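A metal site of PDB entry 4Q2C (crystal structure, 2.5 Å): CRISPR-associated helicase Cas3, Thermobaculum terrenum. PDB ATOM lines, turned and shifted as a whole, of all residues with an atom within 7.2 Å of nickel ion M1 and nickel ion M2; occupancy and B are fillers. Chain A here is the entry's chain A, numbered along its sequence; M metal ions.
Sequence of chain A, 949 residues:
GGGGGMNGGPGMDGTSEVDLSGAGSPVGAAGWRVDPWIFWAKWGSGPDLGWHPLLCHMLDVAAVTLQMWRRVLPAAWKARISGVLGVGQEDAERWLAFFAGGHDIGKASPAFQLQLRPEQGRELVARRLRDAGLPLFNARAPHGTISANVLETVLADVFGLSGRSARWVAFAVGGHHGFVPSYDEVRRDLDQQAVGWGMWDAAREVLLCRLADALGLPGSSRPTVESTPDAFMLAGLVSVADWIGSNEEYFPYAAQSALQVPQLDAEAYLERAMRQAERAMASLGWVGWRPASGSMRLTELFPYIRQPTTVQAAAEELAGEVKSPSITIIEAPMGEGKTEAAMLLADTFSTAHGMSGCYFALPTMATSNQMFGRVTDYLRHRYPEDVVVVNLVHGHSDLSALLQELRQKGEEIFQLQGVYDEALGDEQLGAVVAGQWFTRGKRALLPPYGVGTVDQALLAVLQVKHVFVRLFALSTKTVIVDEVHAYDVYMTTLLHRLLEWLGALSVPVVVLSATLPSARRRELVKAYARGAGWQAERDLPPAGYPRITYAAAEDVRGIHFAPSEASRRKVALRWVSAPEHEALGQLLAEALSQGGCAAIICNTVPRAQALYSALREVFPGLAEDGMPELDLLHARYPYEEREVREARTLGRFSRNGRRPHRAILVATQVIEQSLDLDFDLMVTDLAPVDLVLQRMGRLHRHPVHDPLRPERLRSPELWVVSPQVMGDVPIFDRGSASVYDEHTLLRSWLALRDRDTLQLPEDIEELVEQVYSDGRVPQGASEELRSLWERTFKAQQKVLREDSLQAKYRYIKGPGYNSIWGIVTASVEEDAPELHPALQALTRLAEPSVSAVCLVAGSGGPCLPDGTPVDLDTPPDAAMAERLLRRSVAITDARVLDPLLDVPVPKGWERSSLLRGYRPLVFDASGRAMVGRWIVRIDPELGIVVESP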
ATOM      1  N   ALA A  41      17.318  25.196  15.644  1.00  0.00           N
ATOM      2  CA  ALA A  41      18.250  24.067  15.760  1.00  0.00           C
ATOM      3  C   ALA A  41      18.153  23.134  14.549  1.00  0.00           C
ATOM      4  O   ALA A  41      19.137  22.511  14.162  1.00  0.00           O
ATOM      5  CB  ALA A  41      17.993  23.297  17.039  1.00  0.00           C
ATOM      6  N   LYS A  42      16.967  23.048  13.967  1.00  0.00           N
ATOM      7  CA  LYS A  42      16.750  22.249  12.766  1.00  0.00           C
ATOM      8  C   LYS A  42      16.033  23.091  11.729  1.00  0.00           C
ATOM      9  O   LYS A  42      15.226  23.961  12.062  1.00  0.00           O
ATOM     10  CB  LYS A  42      15.904  21.011  13.073  1.00  0.00           C
ATOM     11  CG  LYS A  42      16.355  20.193  14.263  1.00  0.00           C
ATOM     12  CD  LYS A  42      17.481  19.229  13.912  1.00  0.00           C
ATOM     13  CE  LYS A  42      17.649  18.181  15.007  1.00  0.00           C
ATOM     14  NZ  LYS A  42      18.660  17.145  14.667  1.00  0.00           N
ATOM     15  N   LEU A  54      15.387  25.976  18.685  1.00  0.00           N
ATOM     16  CA  LEU A  54      16.447  25.371  19.491  1.00  0.00           C
ATOM     17  C   LEU A  54      16.004  24.984  20.909  1.00  0.00           C
ATOM     18  O   LEU A  54      16.405  23.945  21.430  1.00  0.00           O
ATOM     19  CB  LEU A  54      17.656  26.291  19.570  1.00  0.00           C
ATOM     20  CG  LEU A  54      18.770  25.948  20.560  1.00  0.00           C
ATOM     21  CD1 LEU A  54      19.439  24.626  20.215  1.00  0.00           C
ATOM     22  CD2 LEU A  54      19.799  27.067  20.660  1.00  0.00           C
ATOM     23  N   HIS A  57      14.286  21.761  20.656  1.00  0.00           N
ATOM     24  CA  HIS A  57      15.192  20.642  20.465  1.00  0.00           C
ATOM     25  C   HIS A  57      15.862  20.249  21.779  1.00  0.00           C
ATOM     26  O   HIS A  57      16.017  19.059  22.076  1.00  0.00           O
ATOM     27  CB  HIS A  57      16.252  20.995  19.414  1.00  0.00           C
ATOM     28  CG  HIS A  57      17.258  19.904  19.195  1.00  0.00           C
ATOM     29  ND1 HIS A  57      16.903  18.633  18.801  1.00  0.00           N
ATOM     30  CD2 HIS A  57      18.612  19.904  19.313  1.00  0.00           C
ATOM     31  CE1 HIS A  57      17.990  17.891  18.691  1.00  0.00           C
ATOM     32  NE2 HIS A  57      19.042  18.633  18.986  1.00  0.00           N
ATOM     33  N   MET A  58      16.242  21.250  22.571  1.00  0.00           N
ATOM     34  CA  MET A  58      16.865  20.978  23.851  1.00  0.00           C
ATOM     35  C   MET A  58      15.876  20.309  24.795  1.00  0.00           C
ATOM     36  O   MET A  58      16.234  19.376  25.533  1.00  0.00           O
ATOM     37  CB  MET A  58      17.405  22.278  24.464  1.00  0.00           C
ATOM     38  CG  MET A  58      18.451  22.961  23.608  1.00  0.00           C
ATOM     39  SD  MET A  58      19.418  24.389  24.532  1.00  0.00           S
ATOM     40  CE  MET A  58      17.947  25.660  24.719  1.00  0.00           C
ATOM     41  N   VAL A  61      15.594  16.557  23.550  1.00  0.00           N
ATOM     42  CA  VAL A  61      16.687  15.700  23.988  1.00  0.00           C
ATOM     43  C   VAL A  61      16.637  15.468  25.497  1.00  0.00           C
ATOM     44  O   VAL A  61      16.913  14.356  25.976  1.00  0.00           O
ATOM     45  CB  VAL A  61      18.058  16.272  23.554  1.00  0.00           C
ATOM     46  CG1 VAL A  61      19.187  15.403  24.047  1.00  0.00           C
ATOM     47  CG2 VAL A  61      18.111  16.404  22.036  1.00  0.00           C
ATOM     48  N   ALA A 100      22.231  16.943  28.663  1.00  0.00           N
ATOM     49  CA  ALA A 100      21.877  16.356  27.367  1.00  0.00           C
ATOM     50  C   ALA A 100      21.106  17.351  26.527  1.00  0.00           C
ATOM     51  O   ALA A 100      21.333  17.467  25.329  1.00  0.00           O
ATOM     52  CB  ALA A 100      21.075  15.082  27.575  1.00  0.00           C
ATOM     53  N   GLY A 101      20.212  18.095  27.167  1.00  0.00           N
ATOM     54  CA  GLY A 101      19.450  19.098  26.447  1.00  0.00           C
ATOM     55  C   GLY A 101      20.375  20.227  26.045  1.00  0.00           C
ATOM     56  O   GLY A 101      20.213  20.839  24.988  1.00  0.00           O
ATOM     57  N   HIS A 103      23.319  20.124  25.083  1.00  0.00           N
ATOM     58  CA  HIS A 103      24.305  19.756  24.065  1.00  0.00           C
ATOM     59  C   HIS A 103      24.385  20.712  22.867  1.00  0.00           C
ATOM     60  O   HIS A 103      25.443  20.866  22.263  1.00  0.00           O
ATOM     61  CB  HIS A 103      23.994  18.364  23.525  1.00  0.00           C
ATOM     62  CG  HIS A 103      22.909  18.348  22.493  1.00  0.00           C
ATOM     63  ND1 HIS A 103      21.583  18.517  22.812  1.00  0.00           N
ATOM     64  CD2 HIS A 103      22.962  18.202  21.145  1.00  0.00           C
ATOM     65  CE1 HIS A 103      20.853  18.461  21.700  1.00  0.00           C
ATOM     66  NE2 HIS A 103      21.671  18.269  20.687  1.00  0.00           N
ATOM     67  N   ASP A 104      23.263  21.345  22.514  1.00  0.00           N
ATOM     68  CA  ASP A 104      23.211  22.190  21.324  1.00  0.00           C
ATOM     69  C   ASP A 104      23.155  23.689  21.624  1.00  0.00           C
ATOM     70  O   ASP A 104      22.724  24.485  20.779  1.00  0.00           O
ATOM     71  CB  ASP A 104      22.029  21.810  20.430  1.00  0.00           C
ATOM     72  CG  ASP A 104      22.447  20.905  19.280  1.00  0.00           C
ATOM     73  OD1 ASP A 104      21.546  20.364  18.617  1.00  0.00           O
ATOM     74  OD2 ASP A 104      23.665  20.744  19.052  1.00  0.00           O
ATOM     75  N   LYS A 107      24.536  26.248  19.236  1.00  0.00           N
ATOM     76  CA  LYS A 107      23.769  26.658  18.070  1.00  0.00           C
ATOM     77  C   LYS A 107      23.260  28.088  18.200  1.00  0.00           C
ATOM     78  O   LYS A 107      22.976  28.749  17.201  1.00  0.00           O
ATOM     79  CB  LYS A 107      22.622  25.684  17.794  1.00  0.00           C
ATOM     80  CG  LYS A 107      23.080  24.348  17.218  1.00  0.00           C
ATOM     81  CD  LYS A 107      21.888  23.467  16.858  1.00  0.00           C
ATOM     82  CE  LYS A 107      22.340  22.185  16.171  1.00  0.00           C
ATOM     83  NZ  LYS A 107      21.192  21.329  15.793  1.00  0.00           N
ATOM     84  N   PHE A 112      26.237  29.760  13.783  1.00  0.00           N
ATOM     85  CA  PHE A 112      25.284  28.722  13.415  1.00  0.00           C
ATOM     86  C   PHE A 112      23.975  29.272  12.868  1.00  0.00           C
ATOM     87  O   PHE A 112      23.427  28.743  11.896  1.00  0.00           O
ATOM     88  CB  PHE A 112      25.006  27.781  14.595  1.00  0.00           C
ATOM     89  CG  PHE A 112      24.191  26.573  14.207  1.00  0.00           C
ATOM     90  CD1 PHE A 112      24.822  25.438  13.732  1.00  0.00           C
ATOM     91  CD2 PHE A 112      22.820  26.584  14.322  1.00  0.00           C
ATOM     92  CE1 PHE A 112      24.087  24.323  13.376  1.00  0.00           C
ATOM     93  CE2 PHE A 112      22.077  25.476  13.956  1.00  0.00           C
ATOM     94  CZ  PHE A 112      22.708  24.341  13.481  1.00  0.00           C
ATOM     95  N   HIS A 143      29.301  23.872  16.103  1.00  0.00           N
ATOM     96  CA  HIS A 143      28.472  24.289  17.226  1.00  0.00           C
ATOM     97  C   HIS A 143      28.748  23.533  18.523  1.00  0.00           C
ATOM     98  O   HIS A 143      28.481  24.054  19.601  1.00  0.00           O
ATOM     99  CB  HIS A 143      26.980  24.242  16.858  1.00  0.00           C
ATOM    100  CG  HIS A 143      26.457  22.863  16.594  1.00  0.00           C
ATOM    101  ND1 HIS A 143      26.483  22.284  15.342  1.00  0.00           N
ATOM    102  CD2 HIS A 143      25.887  21.962  17.421  1.00  0.00           C
ATOM    103  CE1 HIS A 143      25.942  21.083  15.415  1.00  0.00           C
ATOM    104  NE2 HIS A 143      25.571  20.857  16.660  1.00  0.00           N
ATOM    105  N   GLY A 144      29.279  22.322  18.421  1.00  0.00           N
ATOM    106  CA  GLY A 144      29.582  21.539  19.608  1.00  0.00           C
ATOM    107  C   GLY A 144      30.768  22.100  20.378  1.00  0.00           C
ATOM    108  O   GLY A 144      30.785  22.113  21.613  1.00  0.00           O
ATOM    109  N   SER A 147      29.561  24.942  22.115  1.00  0.00           N
ATOM    110  CA  SER A 147      28.783  24.498  23.270  1.00  0.00           C
ATOM    111  C   SER A 147      29.712  24.221  24.429  1.00  0.00           C
ATOM    112  O   SER A 147      29.405  24.574  25.577  1.00  0.00           O
ATOM    113  CB  SER A 147      27.980  23.244  22.933  1.00  0.00           C
ATOM    114  OG  SER A 147      26.838  23.541  22.158  1.00  0.00           O
ATOM    115  N   VAL A 173      29.684  16.768  26.553  1.00  0.00           N
ATOM    116  CA  VAL A 173      28.472  17.167  25.849  1.00  0.00           C
ATOM    117  C   VAL A 173      28.789  17.784  24.492  1.00  0.00           C
ATOM    118  O   VAL A 173      28.038  17.637  23.528  1.00  0.00           O
ATOM    119  CB  VAL A 173      27.635  18.128  26.734  1.00  0.00           C
ATOM    120  CG1 VAL A 173      27.176  19.344  25.950  1.00  0.00           C
ATOM    121  CG2 VAL A 173      26.480  17.392  27.387  1.00  0.00           C
ATOM    122  N   HIS A 176      29.277  15.566  20.962  1.00  0.00           N
ATOM    123  CA  HIS A 176      28.155  14.716  20.538  1.00  0.00           C
ATOM    124  C   HIS A 176      28.138  14.330  19.052  1.00  0.00           C
ATOM    125  O   HIS A 176      27.562  13.315  18.689  1.00  0.00           O
ATOM    126  CB  HIS A 176      26.812  15.337  20.939  1.00  0.00           C
ATOM    127  CG  HIS A 176      26.526  16.645  20.275  1.00  0.00           C
ATOM    128  ND1 HIS A 176      26.851  17.862  20.849  1.00  0.00           N
ATOM    129  CD2 HIS A 176      25.933  16.948  19.094  1.00  0.00           C
ATOM    130  CE1 HIS A 176      26.473  18.847  20.050  1.00  0.00           C
ATOM    131  NE2 HIS A 176      25.915  18.313  18.979  1.00  0.00           N
ATOM    132  N   HIS A 177      28.759  15.140  18.206  1.00  0.00           N
ATOM    133  CA  HIS A 177      28.772  14.858  16.777  1.00  0.00           C
ATOM    134  C   HIS A 177      29.842  13.874  16.294  1.00  0.00           C
ATOM    135  O   HIS A 177      29.912  13.573  15.102  1.00  0.00           O
ATOM    136  CB  HIS A 177      28.794  16.139  15.955  1.00  0.00           C
ATOM    137  CG  HIS A 177      27.465  16.788  15.806  1.00  0.00           C
ATOM    138  ND1 HIS A 177      26.379  16.123  15.275  1.00  0.00           N
ATOM    139  CD2 HIS A 177      27.020  18.023  16.152  1.00  0.00           C
ATOM    140  CE1 HIS A 177      25.321  16.927  15.281  1.00  0.00           C
ATOM    141  NE2 HIS A 177      25.686  18.076  15.809  1.00  0.00           N
ATOM    142  N   VAL A 238      24.537  11.323  25.498  1.00  0.00           N
ATOM    143  CA  VAL A 238      24.086  12.575  24.884  1.00  0.00           C
ATOM    144  C   VAL A 238      23.910  12.407  23.375  1.00  0.00           C
ATOM    145  O   VAL A 238      22.893  12.849  22.812  1.00  0.00           O
ATOM    146  CB  VAL A 238      25.049  13.742  25.199  1.00  0.00           C
ATOM    147  CG1 VAL A 238      24.625  14.994  24.463  1.00  0.00           C
ATOM    148  CG2 VAL A 238      25.105  13.985  26.691  1.00  0.00           C
ATOM    149  N   ALA A 241      20.750  10.379  22.687  1.00  0.00           N
ATOM    150  CA  ALA A 241      19.542  11.155  22.925  1.00  0.00           C
ATOM    151  C   ALA A 241      19.302  12.154  21.793  1.00  0.00           C
ATOM    152  O   ALA A 241      18.163  12.392  21.391  1.00  0.00           O
ATOM    153  CB  ALA A 241      19.616  11.857  24.263  1.00  0.00           C
ATOM    154  N   ASP A 242      20.385  12.696  21.249  1.00  0.00           N
ATOM    155  CA  ASP A 242      20.249  13.575  20.087  1.00  0.00           C
ATOM    156  C   ASP A 242      19.745  12.834  18.845  1.00  0.00           C
ATOM    157  O   ASP A 242      18.933  13.363  18.078  1.00  0.00           O
ATOM    158  CB  ASP A 242      21.557  14.300  19.794  1.00  0.00           C
ATOM    159  CG  ASP A 242      21.430  15.284  18.645  1.00  0.00           C
ATOM    160  OD1 ASP A 242      22.044  15.062  17.588  1.00  0.00           O
ATOM    161  OD2 ASP A 242      20.705  16.286  18.809  1.00  0.00           O
ATOM    162  N   TRP A 243      20.202  11.592  18.658  1.00  0.00           N
ATOM    163  CA  TRP A 243      19.720  10.786  17.538  1.00  0.00           C
ATOM    164  C   TRP A 243      18.226  10.519  17.675  1.00  0.00           C
ATOM    165  O   TRP A 243      17.469  10.627  16.704  1.00  0.00           O
ATOM    166  CB  TRP A 243      20.460   9.450  17.433  1.00  0.00           C
ATOM    167  CG  TRP A 243      21.927   9.579  17.144  1.00  0.00           C
ATOM    168  CD1 TRP A 243      22.579  10.665  16.652  1.00  0.00           C
ATOM    169  CD2 TRP A 243      22.924   8.569  17.360  1.00  0.00           C
ATOM    170  NE1 TRP A 243      23.924  10.402  16.540  1.00  0.00           N
ATOM    171  CE2 TRP A 243      24.156   9.121  16.971  1.00  0.00           C
ATOM    172  CE3 TRP A 243      22.884   7.261  17.843  1.00  0.00           C
ATOM    173  CZ2 TRP A 243      25.362   8.400  17.046  1.00  0.00           C
ATOM    174  CZ3 TRP A 243      24.070   6.544  17.927  1.00  0.00           C
ATOM    175  CH2 TRP A 243      25.289   7.118  17.521  1.00  0.00           C
ATOM    176  N   GLY A 245      16.188  12.399  19.203  1.00  0.00           N
ATOM    177  CA  GLY A 245      15.522  13.674  19.027  1.00  0.00           C
ATOM    178  C   GLY A 245      15.524  14.140  17.581  1.00  0.00           C
ATOM    179  O   GLY A 245      14.836  15.102  17.232  1.00  0.00           O
ATOM    180  N   SER A 246      16.304  13.471  16.733  1.00  0.00           N
ATOM    181  CA  SER A 246      16.393  13.863  15.333  1.00  0.00           C
ATOM    182  C   SER A 246      15.441  13.114  14.396  1.00  0.00           C
ATOM    183  O   SER A 246      15.462  13.331  13.174  1.00  0.00           O
ATOM    184  CB  SER A 246      17.835  13.749  14.838  1.00  0.00           C
ATOM    185  OG  SER A 246      18.668  14.684  15.516  1.00  0.00           O
ATOM    186  N   GLY A 418      18.469  16.236   9.806  1.00  0.00           N
ATOM    187  CA  GLY A 418      18.932  17.430  10.480  1.00  0.00           C
ATOM    188  C   GLY A 418      19.993  17.175  11.531  1.00  0.00           C
ATOM    189  O   GLY A 418      19.983  17.798  12.588  1.00  0.00           O
ATOM    190  N   VAL A 419      20.883  16.224  11.272  1.00  0.00           N
ATOM    191  CA  VAL A 419      22.043  16.034  12.136  1.00  0.00           C
ATOM    192  C   VAL A 419      23.196  16.858  11.584  1.00  0.00           C
ATOM    193  O   VAL A 419      23.807  16.498  10.569  1.00  0.00           O
ATOM    194  CB  VAL A 419      22.446  14.555  12.249  1.00  0.00           C
ATOM    195  CG1 VAL A 419      23.734  14.410  13.043  1.00  0.00           C
ATOM    196  CG2 VAL A 419      21.309  13.757  12.897  1.00  0.00           C
ATOM    197  N   TYR A 420      23.490  17.977  12.239  1.00  0.00           N
ATOM    198  CA  TYR A 420      24.411  18.976  11.702  1.00  0.00           C
ATOM    199  C   TYR A 420      25.870  18.668  12.019  1.00  0.00           C
ATOM    200  O   TYR A 420      26.530  19.445  12.725  1.00  0.00           O
ATOM    201  CB  TYR A 420      24.026  20.376  12.182  1.00  0.00           C
ATOM    202  CG  TYR A 420      22.782  20.911  11.514  1.00  0.00           C
ATOM    203  CD1 TYR A 420      21.542  20.350  11.752  1.00  0.00           C
ATOM    204  CD2 TYR A 420      22.852  21.984  10.626  1.00  0.00           C
ATOM    205  CE1 TYR A 420      20.401  20.826  11.136  1.00  0.00           C
ATOM    206  CE2 TYR A 420      21.718  22.477  10.017  1.00  0.00           C
ATOM    207  CZ  TYR A 420      20.496  21.882  10.268  1.00  0.00           C
ATOM    208  OH  TYR A 420      19.369  22.366   9.646  1.00  0.00           O
ATOM    209  N   ASP A 421      26.371  17.552  11.507  1.00  0.00           N
ATOM    210  CA  ASP A 421      27.775  17.200  11.696  1.00  0.00           C
ATOM    211  C   ASP A 421      28.656  18.214  10.976  1.00  0.00           C
ATOM    212  O   ASP A 421      28.439  18.515   9.804  1.00  0.00           O
ATOM    213  CB  ASP A 421      28.043  15.800  11.154  1.00  0.00           C
ATOM    214  CG  ASP A 421      29.295  15.167  11.740  1.00  0.00           C
ATOM    215  OD1 ASP A 421      30.288  15.887  11.944  1.00  0.00           O
ATOM    216  OD2 ASP A 421      29.277  13.944  11.998  1.00  0.00           O
HETATM  217 NI    NI M   1      20.992  18.314  18.576  1.00  0.00          NI
HETATM  218 NI    NI M   2      24.630  19.198  17.501  1.00  0.00          NI
HETATM  219 NI    NI M   3      22.141  18.088  16.051  1.00  0.00          NI
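Nickel ion M2 is bound by a ring nitrogen (NE2) of His 143. A ring nitrogen (NE2) of His 176 binds nickel ion M2, at 2.1 Å. NE2 of His 177 binds nickel ion M2, 2.3 Å away. OD2 of Asp 104 binds nickel ion M2 (2.4 Å).
Nickel ion M1 is bound by a ring nitrogen (NE2) of His 57 (2.0 Å), the side-chain carboxylate of Asp 242 (2.1 Å), the side-chain carboxylate of Asp 104 (2.1 Å) and a ring nitrogen (NE2) of His 103 (2.2 Å).
Of the 28 residues printed, 4 come within 4 Å of nickel ion M1.
Merely in contact with nickel ion M2: Lys 107. Five residues have an atom within 4 Å of nickel ion M2: Asp 104, Lys 107, His 143, His 176 and His 177. Along chain A the residues within 4 Å of nickel ion M2 span positions 104 to 177. The nearest printed residue that does not touch nickel ion M2 is His 103 (4.1 Å).
The side-chain amino group (NZ) of Lys 107 is in hydrogen-bond range of the backbone carbonyl oxygen (O) of Ala 41, 2.9 Å away. The backbone carbonyl oxygen (O) of Tyr 420 sits close to a ring nitrogen (NE2) of His 177 (3.5 Å). O of His 143 sits at hydrogen-bond distance from OG of Ser 147 (3.1 Å). A ring nitrogen (ND1) of His 103 sits at hydrogen-bond distance from the backbone carbonyl oxygen (O) of Ala 100. ND1 of His 103 lies within hydrogen-bond range of O of Gly 101, 3.5 Å away. O of His 103 lies within hydrogen-bond range of OG of Ser 147 (3.0 Å). The side-chain carboxylate (OD1) of Asp 104 lies close to the side-chain amino group (NZ) of Lys 107, 3.0 Å away. The side-chain hydroxyl of Ser 246 lies within hydrogen-bond range of the backbone carbonyl oxygen of Asp 242 (2.9 Å).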
